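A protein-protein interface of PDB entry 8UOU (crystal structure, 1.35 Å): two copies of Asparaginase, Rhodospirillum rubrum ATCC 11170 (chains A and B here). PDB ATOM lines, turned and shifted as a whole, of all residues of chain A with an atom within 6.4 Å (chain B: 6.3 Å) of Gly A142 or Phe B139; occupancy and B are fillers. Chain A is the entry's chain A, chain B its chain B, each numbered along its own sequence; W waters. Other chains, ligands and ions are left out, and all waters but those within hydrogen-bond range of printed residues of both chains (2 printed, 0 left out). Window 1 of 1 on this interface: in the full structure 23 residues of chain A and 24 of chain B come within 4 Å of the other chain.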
ATOM      1  N   VAL A  51     -15.003  32.211   2.638  1.00  0.00           N
ATOM      2  CA  VAL A  51     -15.380  30.798   2.608  1.00  0.00           C
ATOM      3  C   VAL A  51     -16.185  30.522   1.367  1.00  0.00           C
ATOM      4  O   VAL A  51     -15.943  29.499   0.654  1.00  0.00           O
ATOM      5  CB  VAL A  51     -16.148  30.365   3.876  1.00  0.00           C
ATOM      6  CG1 VAL A  51     -16.600  28.926   3.819  1.00  0.00           C
ATOM      7  CG2 VAL A  51     -15.314  30.603   5.129  1.00  0.00           C
ATOM      8  N   LEU A  52     -17.141  31.331   1.020  1.00  0.00           N
ATOM      9  CA  LEU A  52     -17.998  31.051  -0.137  1.00  0.00           C
ATOM     10  C   LEU A  52     -17.220  31.209  -1.454  1.00  0.00           C
ATOM     11  O   LEU A  52     -17.592  30.529  -2.434  1.00  0.00           O
ATOM     12  CB  LEU A  52     -19.270  31.864  -0.139  1.00  0.00           C
ATOM     13  CG  LEU A  52     -20.193  31.594   1.024  1.00  0.00           C
ATOM     14  CD1 LEU A  52     -21.521  32.300   0.756  1.00  0.00           C
ATOM     15  CD2 LEU A  52     -20.436  30.133   1.343  1.00  0.00           C
ATOM     16  N   THR A  54     -14.473  29.908  -2.330  1.00  0.00           N
ATOM     17  CA  THR A  54     -13.879  28.614  -2.732  1.00  0.00           C
ATOM     18  C   THR A  54     -14.833  27.465  -2.443  1.00  0.00           C
ATOM     19  O   THR A  54     -14.442  26.292  -2.667  1.00  0.00           O
ATOM     20  CB  THR A  54     -12.576  28.425  -1.982  1.00  0.00           C
ATOM     21  OG1 THR A  54     -12.799  28.512  -0.572  1.00  0.00           O
ATOM     22  CG2 THR A  54     -11.523  29.398  -2.444  1.00  0.00           C
ATOM     23  N   ALA A  55     -16.108  27.704  -2.220  1.00  0.00           N
ATOM     24  CA  ALA A  55     -17.067  26.636  -1.889  1.00  0.00           C
ATOM     25  C   ALA A  55     -17.612  25.926  -3.151  1.00  0.00           C
ATOM     26  O   ALA A  55     -18.397  24.991  -2.986  1.00  0.00           O
ATOM     27  CB  ALA A  55     -18.178  27.208  -1.034  1.00  0.00           C
ATOM     28  N   LEU A  57     -19.988  26.766  -5.163  1.00  0.00           N
ATOM     29  CA  LEU A  57     -21.463  26.742  -5.066  1.00  0.00           C
ATOM     30  C   LEU A  57     -22.152  26.539  -6.422  1.00  0.00           C
ATOM     31  O   LEU A  57     -21.693  27.076  -7.448  1.00  0.00           O
ATOM     32  CB  LEU A  57     -21.947  28.042  -4.437  1.00  0.00           C
ATOM     33  CG  LEU A  57     -21.440  28.319  -3.030  1.00  0.00           C
ATOM     34  CD1 LEU A  57     -21.943  29.672  -2.582  1.00  0.00           C
ATOM     35  CD2 LEU A  57     -21.831  27.248  -2.045  1.00  0.00           C
ATOM     36  N   ALA A 137     -14.407  28.474  11.792  1.00  0.00           N
ATOM     37  CA  ALA A 137     -15.285  29.318  10.957  1.00  0.00           C
ATOM     38  C   ALA A 137     -15.798  28.588   9.708  1.00  0.00           C
ATOM     39  O   ALA A 137     -16.997  28.666   9.407  1.00  0.00           O
ATOM     40  CB  ALA A 137     -14.578  30.590  10.540  1.00  0.00           C
ATOM     41  N   ALA A 138     -14.926  27.959   8.898  1.00  0.00           N
ATOM     42  CA  ALA A 138     -15.382  27.372   7.614  1.00  0.00           C
ATOM     43  C   ALA A 138     -16.394  26.244   7.848  1.00  0.00           C
ATOM     44  O   ALA A 138     -17.440  26.186   7.166  1.00  0.00           O
ATOM     45  CB  ALA A 138     -14.204  26.946   6.795  1.00  0.00           C
ATOM     46  N   PHE A 139     -16.092  25.378   8.782  1.00  0.00           N
ATOM     47  CA  PHE A 139     -17.043  24.326   9.168  1.00  0.00           C
ATOM     48  C   PHE A 139     -18.379  24.958   9.559  1.00  0.00           C
ATOM     49  O   PHE A 139     -19.443  24.526   9.190  1.00  0.00           O
ATOM     50  CB  PHE A 139     -16.481  23.480  10.316  1.00  0.00           C
ATOM     51  CG  PHE A 139     -17.431  22.446  10.852  1.00  0.00           C
ATOM     52  CD1 PHE A 139     -17.542  21.185  10.259  1.00  0.00           C
ATOM     53  CD2 PHE A 139     -18.267  22.750  11.882  1.00  0.00           C
ATOM     54  CE1 PHE A 139     -18.471  20.269  10.726  1.00  0.00           C
ATOM     55  CE2 PHE A 139     -19.217  21.861  12.338  1.00  0.00           C
ATOM     56  CZ  PHE A 139     -19.298  20.615  11.762  1.00  0.00           C
ATOM     57  N   ASN A 140     -18.296  25.965  10.440  1.00  0.00           N
ATOM     58  CA  ASN A 140     -19.522  26.591  10.963  1.00  0.00           C
ATOM     59  C   ASN A 140     -20.336  27.215   9.854  1.00  0.00           C
ATOM     60  O   ASN A 140     -21.584  27.139   9.872  1.00  0.00           O
ATOM     61  CB  ASN A 140     -19.254  27.658  12.028  1.00  0.00           C
ATOM     62  CG  ASN A 140     -18.647  27.124  13.275  1.00  0.00           C
ATOM     63  OD1 ASN A 140     -18.697  25.943  13.578  1.00  0.00           O
ATOM     64  ND2 ASN A 140     -18.137  28.044  14.091  1.00  0.00           N
ATOM     65  N   ILE A 141     -19.668  27.819   8.891  1.00  0.00           N
ATOM     66  CA  ILE A 141     -20.408  28.415   7.762  1.00  0.00           C
ATOM     67  C   ILE A 141     -21.126  27.299   6.948  1.00  0.00           C
ATOM     68  O   ILE A 141     -22.275  27.479   6.547  1.00  0.00           O
ATOM     69  CB  ILE A 141     -19.452  29.272   6.907  1.00  0.00           C
ATOM     70  CG1 ILE A 141     -19.016  30.521   7.687  1.00  0.00           C
ATOM     71  CG2 ILE A 141     -20.063  29.648   5.569  1.00  0.00           C
ATOM     72  CD1 ILE A 141     -20.113  31.411   8.223  1.00  0.00           C
ATOM     73  N   GLY A 142     -20.400  26.243   6.617  1.00  0.00           N
ATOM     74  CA  GLY A 142     -21.058  25.172   5.872  1.00  0.00           C
ATOM     75  C   GLY A 142     -22.255  24.622   6.619  1.00  0.00           C
ATOM     76  O   GLY A 142     -23.342  24.432   6.044  1.00  0.00           O
ATOM     77  N   PHE A 143     -22.045  24.338   7.909  1.00  0.00           N
ATOM     78  CA  PHE A 143     -23.128  23.767   8.706  1.00  0.00           C
ATOM     79  C   PHE A 143     -24.333  24.717   8.735  1.00  0.00           C
ATOM     80  O   PHE A 143     -25.477  24.329   8.686  1.00  0.00           O
ATOM     81  CB  PHE A 143     -22.596  23.447  10.091  1.00  0.00           C
ATOM     82  CG  PHE A 143     -23.508  22.619  10.940  1.00  0.00           C
ATOM     83  CD1 PHE A 143     -24.511  23.243  11.698  1.00  0.00           C
ATOM     84  CD2 PHE A 143     -23.314  21.248  11.052  1.00  0.00           C
ATOM     85  CE1 PHE A 143     -25.366  22.469  12.469  1.00  0.00           C
ATOM     86  CE2 PHE A 143     -24.147  20.482  11.835  1.00  0.00           C
ATOM     87  CZ  PHE A 143     -25.197  21.086  12.503  1.00  0.00           C
ATOM     88  N   ALA A 144     -24.020  26.013   8.960  1.00  0.00           N
ATOM     89  CA  ALA A 144     -25.066  27.021   9.127  1.00  0.00           C
ATOM     90  C   ALA A 144     -25.803  27.306   7.838  1.00  0.00           C
ATOM     91  O   ALA A 144     -27.024  27.569   7.855  1.00  0.00           O
ATOM     92  CB  ALA A 144     -24.521  28.304   9.736  1.00  0.00           C
ATOM     93  N   CYS A 145     -25.125  27.226   6.691  1.00  0.00           N
ATOM     94  CA  CYS A 145     -25.800  27.359   5.388  1.00  0.00           C
ATOM     95  C   CYS A 145     -26.792  26.208   5.168  1.00  0.00           C
ATOM     96  O   CYS A 145     -27.928  26.436   4.767  1.00  0.00           O
ATOM     97  CB  CYS A 145     -24.807  27.410   4.232  1.00  0.00           C
ATOM     98  SG  CYS A 145     -23.903  28.974   4.059  1.00  0.00           S
ATOM     99  N   ALA A 146     -26.364  24.987   5.514  1.00  0.00           N
ATOM    100  CA  ALA A 146     -27.274  23.846   5.435  1.00  0.00           C
ATOM    101  C   ALA A 146     -28.464  24.026   6.358  1.00  0.00           C
ATOM    102  O   ALA A 146     -29.635  23.822   5.963  1.00  0.00           O
ATOM    103  CB  ALA A 146     -26.576  22.563   5.704  1.00  0.00           C
ATOM    104  N   ALA A 147     -28.194  24.471   7.606  1.00  0.00           N
ATOM    105  CA  ALA A 147     -29.280  24.664   8.579  1.00  0.00           C
ATOM    106  C   ALA A 147     -30.267  25.733   8.073  1.00  0.00           C
ATOM    107  O   ALA A 147     -31.490  25.502   8.166  1.00  0.00           O
ATOM    108  CB  ALA A 147     -28.741  25.107   9.920  1.00  0.00           C
ATOM    109  N   VAL B  51     -10.697  18.715  10.028  1.00  0.00           N
ATOM    110  CA  VAL B  51     -11.750  19.735  10.159  1.00  0.00           C
ATOM    111  C   VAL B  51     -12.471  19.568  11.478  1.00  0.00           C
ATOM    112  O   VAL B  51     -12.745  20.575  12.187  1.00  0.00           O
ATOM    113  CB  VAL B  51     -12.714  19.675   8.973  1.00  0.00           C
ATOM    114  CG1 VAL B  51     -13.836  20.663   9.128  1.00  0.00           C
ATOM    115  CG2 VAL B  51     -11.962  19.863   7.681  1.00  0.00           C
ATOM    116  N   SER B 135      -9.365  25.088  -0.951  1.00  0.00           N
ATOM    117  CA  SER B 135     -10.228  23.914  -1.001  1.00  0.00           C
ATOM    118  C   SER B 135     -11.629  24.189  -0.527  1.00  0.00           C
ATOM    119  O   SER B 135     -11.853  24.935   0.485  1.00  0.00           O
ATOM    120  CB  SER B 135      -9.636  22.791  -0.193  1.00  0.00           C
ATOM    121  OG  SER B 135     -10.515  21.679  -0.112  1.00  0.00           O
ATOM    122  N   ASP B 136     -12.625  23.582  -1.123  1.00  0.00           N
ATOM    123  CA  ASP B 136     -14.039  23.486  -0.710  1.00  0.00           C
ATOM    124  C   ASP B 136     -14.278  22.526   0.466  1.00  0.00           C
ATOM    125  O   ASP B 136     -15.393  22.439   0.953  1.00  0.00           O
ATOM    126  CB  ASP B 136     -14.850  23.007  -1.957  1.00  0.00           C
ATOM    127  CG  ASP B 136     -14.342  21.776  -2.779  1.00  0.00           C
ATOM    128  OD1 ASP B 136     -13.120  21.630  -2.892  1.00  0.00           O
ATOM    129  OD2 ASP B 136     -15.216  21.023  -3.260  1.00  0.00           O
ATOM    130  N   ALA B 137     -13.265  21.784   0.899  1.00  0.00           N
ATOM    131  CA  ALA B 137     -13.469  20.640   1.812  1.00  0.00           C
ATOM    132  C   ALA B 137     -14.121  21.045   3.125  1.00  0.00           C
ATOM    133  O   ALA B 137     -15.061  20.401   3.544  1.00  0.00           O
ATOM    134  CB  ALA B 137     -12.170  19.955   2.076  1.00  0.00           C
ATOM    135  N   ALA B 138     -13.605  22.049   3.848  1.00  0.00           N
ATOM    136  CA  ALA B 138     -14.145  22.360   5.200  1.00  0.00           C
ATOM    137  C   ALA B 138     -15.620  22.813   5.127  1.00  0.00           C
ATOM    138  O   ALA B 138     -16.477  22.339   5.890  1.00  0.00           O
ATOM    139  CB  ALA B 138     -13.318  23.397   5.888  1.00  0.00           C
ATOM    140  N   PHE B 139     -15.927  23.656   4.134  1.00  0.00           N
ATOM    141  CA  PHE B 139     -17.319  24.051   3.921  1.00  0.00           C
ATOM    142  C   PHE B 139     -18.170  22.806   3.688  1.00  0.00           C
ATOM    143  O   PHE B 139     -19.263  22.656   4.182  1.00  0.00           O
ATOM    144  CB  PHE B 139     -17.455  25.030   2.726  1.00  0.00           C
ATOM    145  CG  PHE B 139     -18.859  25.394   2.356  1.00  0.00           C
ATOM    146  CD1 PHE B 139     -19.498  26.468   2.956  1.00  0.00           C
ATOM    147  CD2 PHE B 139     -19.525  24.644   1.430  1.00  0.00           C
ATOM    148  CE1 PHE B 139     -20.816  26.771   2.624  1.00  0.00           C
ATOM    149  CE2 PHE B 139     -20.830  24.916   1.124  1.00  0.00           C
ATOM    150  CZ  PHE B 139     -21.476  25.996   1.723  1.00  0.00           C
ATOM    151  N   ASN B 140     -17.700  21.949   2.737  1.00  0.00           N
ATOM    152  CA  ASN B 140     -18.459  20.770   2.368  1.00  0.00           C
ATOM    153  C   ASN B 140     -18.696  19.879   3.558  1.00  0.00           C
ATOM    154  O   ASN B 140     -19.803  19.301   3.661  1.00  0.00           O
ATOM    155  CB  ASN B 140     -17.822  19.959   1.231  1.00  0.00           C
ATOM    156  CG  ASN B 140     -17.752  20.690  -0.083  1.00  0.00           C
ATOM    157  OD1 ASN B 140     -18.492  21.659  -0.322  1.00  0.00           O
ATOM    158  ND2 ASN B 140     -16.921  20.121  -0.990  1.00  0.00           N
ATOM    159  N   ILE B 141     -17.702  19.690   4.403  1.00  0.00           N
ATOM    160  CA  ILE B 141     -17.870  18.869   5.604  1.00  0.00           C
ATOM    161  C   ILE B 141     -18.918  19.463   6.537  1.00  0.00           C
ATOM    162  O   ILE B 141     -19.797  18.720   7.027  1.00  0.00           O
ATOM    163  CB  ILE B 141     -16.519  18.670   6.300  1.00  0.00           C
ATOM    164  CG1 ILE B 141     -15.631  17.756   5.456  1.00  0.00           C
ATOM    165  CG2 ILE B 141     -16.692  18.091   7.704  1.00  0.00           C
ATOM    166  CD1 ILE B 141     -14.168  17.915   5.756  1.00  0.00           C
ATOM    167  N   GLY B 142     -18.886  20.754   6.785  1.00  0.00           N
ATOM    168  CA  GLY B 142     -19.903  21.388   7.656  1.00  0.00           C
ATOM    169  C   GLY B 142     -21.308  21.216   7.094  1.00  0.00           C
ATOM    170  O   GLY B 142     -22.228  20.766   7.768  1.00  0.00           O
ATOM    171  N   PHE B 143     -21.425  21.501   5.801  1.00  0.00           N
ATOM    172  CA  PHE B 143     -22.726  21.414   5.136  1.00  0.00           C
ATOM    173  C   PHE B 143     -23.270  19.980   5.183  1.00  0.00           C
ATOM    174  O   PHE B 143     -24.456  19.718   5.433  1.00  0.00           O
ATOM    175  CB  PHE B 143     -22.588  21.934   3.681  1.00  0.00           C
ATOM    176  CG  PHE B 143     -23.881  22.085   2.937  1.00  0.00           C
ATOM    177  CD1 PHE B 143     -24.507  20.987   2.323  1.00  0.00           C
ATOM    178  CD2 PHE B 143     -24.484  23.312   2.864  1.00  0.00           C
ATOM    179  CE1 PHE B 143     -25.742  21.161   1.714  1.00  0.00           C
ATOM    180  CE2 PHE B 143     -25.703  23.465   2.240  1.00  0.00           C
ATOM    181  CZ  PHE B 143     -26.314  22.395   1.624  1.00  0.00           C
ATOM    182  N   ALA B 144     -22.362  19.015   4.916  1.00  0.00           N
ATOM    183  CA  ALA B 144     -22.751  17.583   4.854  1.00  0.00           C
ATOM    184  C   ALA B 144     -23.067  17.010   6.197  1.00  0.00           C
ATOM    185  O   ALA B 144     -23.956  16.156   6.318  1.00  0.00           O
ATOM    186  CB  ALA B 144     -21.701  16.795   4.148  1.00  0.00           C
ATOM    187  N   ALA B 146     -24.459  18.746   8.674  1.00  0.00           N
ATOM    188  CA  ALA B 146     -25.829  19.234   8.913  1.00  0.00           C
ATOM    189  C   ALA B 146     -26.835  18.430   8.113  1.00  0.00           C
ATOM    190  O   ALA B 146     -27.856  18.007   8.610  1.00  0.00           O
ATOM    191  CB  ALA B 146     -25.919  20.698   8.584  1.00  0.00           C
ATOM    192  N   HIS B 160     -21.544  21.486  -3.382  1.00  0.00           N
ATOM    193  CA  HIS B 160     -21.873  22.763  -4.036  1.00  0.00           C
ATOM    194  C   HIS B 160     -22.942  23.555  -3.222  1.00  0.00           C
ATOM    195  O   HIS B 160     -23.723  24.330  -3.808  1.00  0.00           O
ATOM    196  CB  HIS B 160     -22.369  22.567  -5.466  1.00  0.00           C
ATOM    197  CG  HIS B 160     -21.508  21.633  -6.279  1.00  0.00           C
ATOM    198  ND1 HIS B 160     -20.173  21.817  -6.458  1.00  0.00           N
ATOM    199  CD2 HIS B 160     -21.805  20.508  -6.948  1.00  0.00           C
ATOM    200  CE1 HIS B 160     -19.665  20.787  -7.200  1.00  0.00           C
ATOM    201  NE2 HIS B 160     -20.661  20.013  -7.490  1.00  0.00           N
ATOM    202  N   GLY B 161     -23.032  23.281  -1.911  1.00  0.00           N
ATOM    203  CA  GLY B 161     -24.024  23.961  -1.063  1.00  0.00           C
ATOM    204  C   GLY B 161     -25.450  23.571  -1.333  1.00  0.00           C
ATOM    205  O   GLY B 161     -26.348  24.354  -1.083  1.00  0.00           O
ATOM    206  N   LYS B 162     -25.655  22.379  -1.882  1.00  0.00           N
ATOM    207  CA  LYS B 162     -27.021  21.890  -2.103  1.00  0.00           C
ATOM    208  C   LYS B 162     -27.042  20.364  -2.038  1.00  0.00           C
ATOM    209  O   LYS B 162     -26.021  19.723  -1.831  1.00  0.00           O
ATOM    210  CB  LYS B 162     -27.585  22.426  -3.387  1.00  0.00           C
ATOM    211  CG  LYS B 162     -26.807  21.874  -4.555  1.00  0.00           C
ATOM    212  CD  LYS B 162     -27.542  22.135  -5.919  1.00  0.00           C
ATOM    213  CE  LYS B 162     -28.700  21.182  -6.070  1.00  0.00           C
ATOM    214  NZ  LYS B 162     -29.310  21.275  -7.390  1.00  0.00           N
HETATM  215  O   HOH W   1     -10.479  27.265   1.335  1.00  0.00           O
HETATM  216  O   HOH W   2     -18.872  22.334  -2.928  1.00  0.00           O
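OG of Ser B135 sits at hydrogen-bond distance from N of Ala B137. The side-chain carboxylate of Asp B136 is in hydrogen-bond range of the side-chain amide nitrogen of Asn B140.
Water W2 lies within hydrogen-bond range of O of Ala A55 (2.7 Å), OD1 of Asn B140 (2.7 Å) and N of His B160 (2.8 Å). Water W1 bridges the backbone carbonyl oxygen (O) of Ser B135 (2.8 Å) and the side-chain hydroxyl (OG1) of Thr A54 (3.3 Å).
Ala A138 touches its own counterpart, Ala B138. Phe A139 touches Gly B142, and with the chains exchanged Gly A142 touches Phe B139. Phe A143 touches its own counterpart, Phe B143. Ala A146 touches its own counterpart, Ala B146. 10 positions are printed for both chains. Of the 20 pairs that touch across the chains among the printed residues, 14 have their exchanged pair printed and touching as well.
Among the printed residues, merely in contact across the chains: Gly A142 with Phe B143 (3.2 Å), Phe A143 with Gly B142 (3.3 Å), Thr A54 with Asp B136 (3.4 Å), Ala A146 with Ala B146 (3.5 Å), Phe A139 with Gly B142 (3.5 Å), Gly A142 with Phe B139 (3.5 Å), Leu A57 with His B160 (3.5 Å), Ala A146 with Phe B143 (3.6 Å), Gly A142 with Gly B142 (3.6 Å), Phe A143 with Phe B143 (3.6 Å), Phe A143 with Ala B146 (3.6 Å), Leu A52 with Phe B139 (3.6 Å), Ala A138 with Ala B138 (3.8 Å), Ala A55 with Phe B139 (3.8 Å), Thr A54 with Ser B135 (3.8 Å), Phe A139 with Ala B138 (3.9 Å), Ala A138 with Phe B139 (3.9 Å), Val A51 with Phe B139 (3.9 Å), Phe A139 with Val B51 (3.9 Å) and Leu A57 with Phe B139 (3.99 Å).
Hydrophobic or aromatic side chains of chain A that line the printed part of chain B: Val A51, Leu A52, Ala A55, Leu A57, Ala A138, Phe A139, Phe A143 and Ala A146. Printed residues of chain B that touch a printed residue of chain A: Val B51, Ser B135, Asp B136, Ala B138, Phe B139, Gly B142, Phe B143, Ala B146 and His B160. Hydrophobic or aromatic side chains of chain B that line the printed part of chain A: Val B51, Ala B138, Phe B139, Phe B143 and Ala B146. Among the printed residues, 20 pairs touch across the chains. Among the printed residues, no Asp or Glu carboxylate lies within 4 Å of a Lys or Arg side-chain nitrogen of the other chain.
Gly A142 touches just these residues of chain B: Phe B139, Gly B142 and Phe B143. Printed residues of chain B within 4 Å of Phe A139: Val B51 (3.9 Å), Ala B138 (3.9 Å) and Gly B142 (3.5 Å). Of the printed residues of chain B, Phe A143 touches Gly B142, Phe B143 and Ala B146. Of the printed residues of chain B, Val A51 touches Phe B139. Of the printed residues of chain B, Leu A52 touches Phe B139. Printed residues of chain B within 4 Å of Ala A55: Phe B139. Cys A145 touches none of the printed residues of chain B. Asn A140 touches none of the printed residues of chain B. The nearest residue of chain B that does not touch Gly A142 is Ala B146 (5.2 Å). The nearest printed residue of chain B that does not touch Ala A146 is Gly B142 (5.1 Å).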
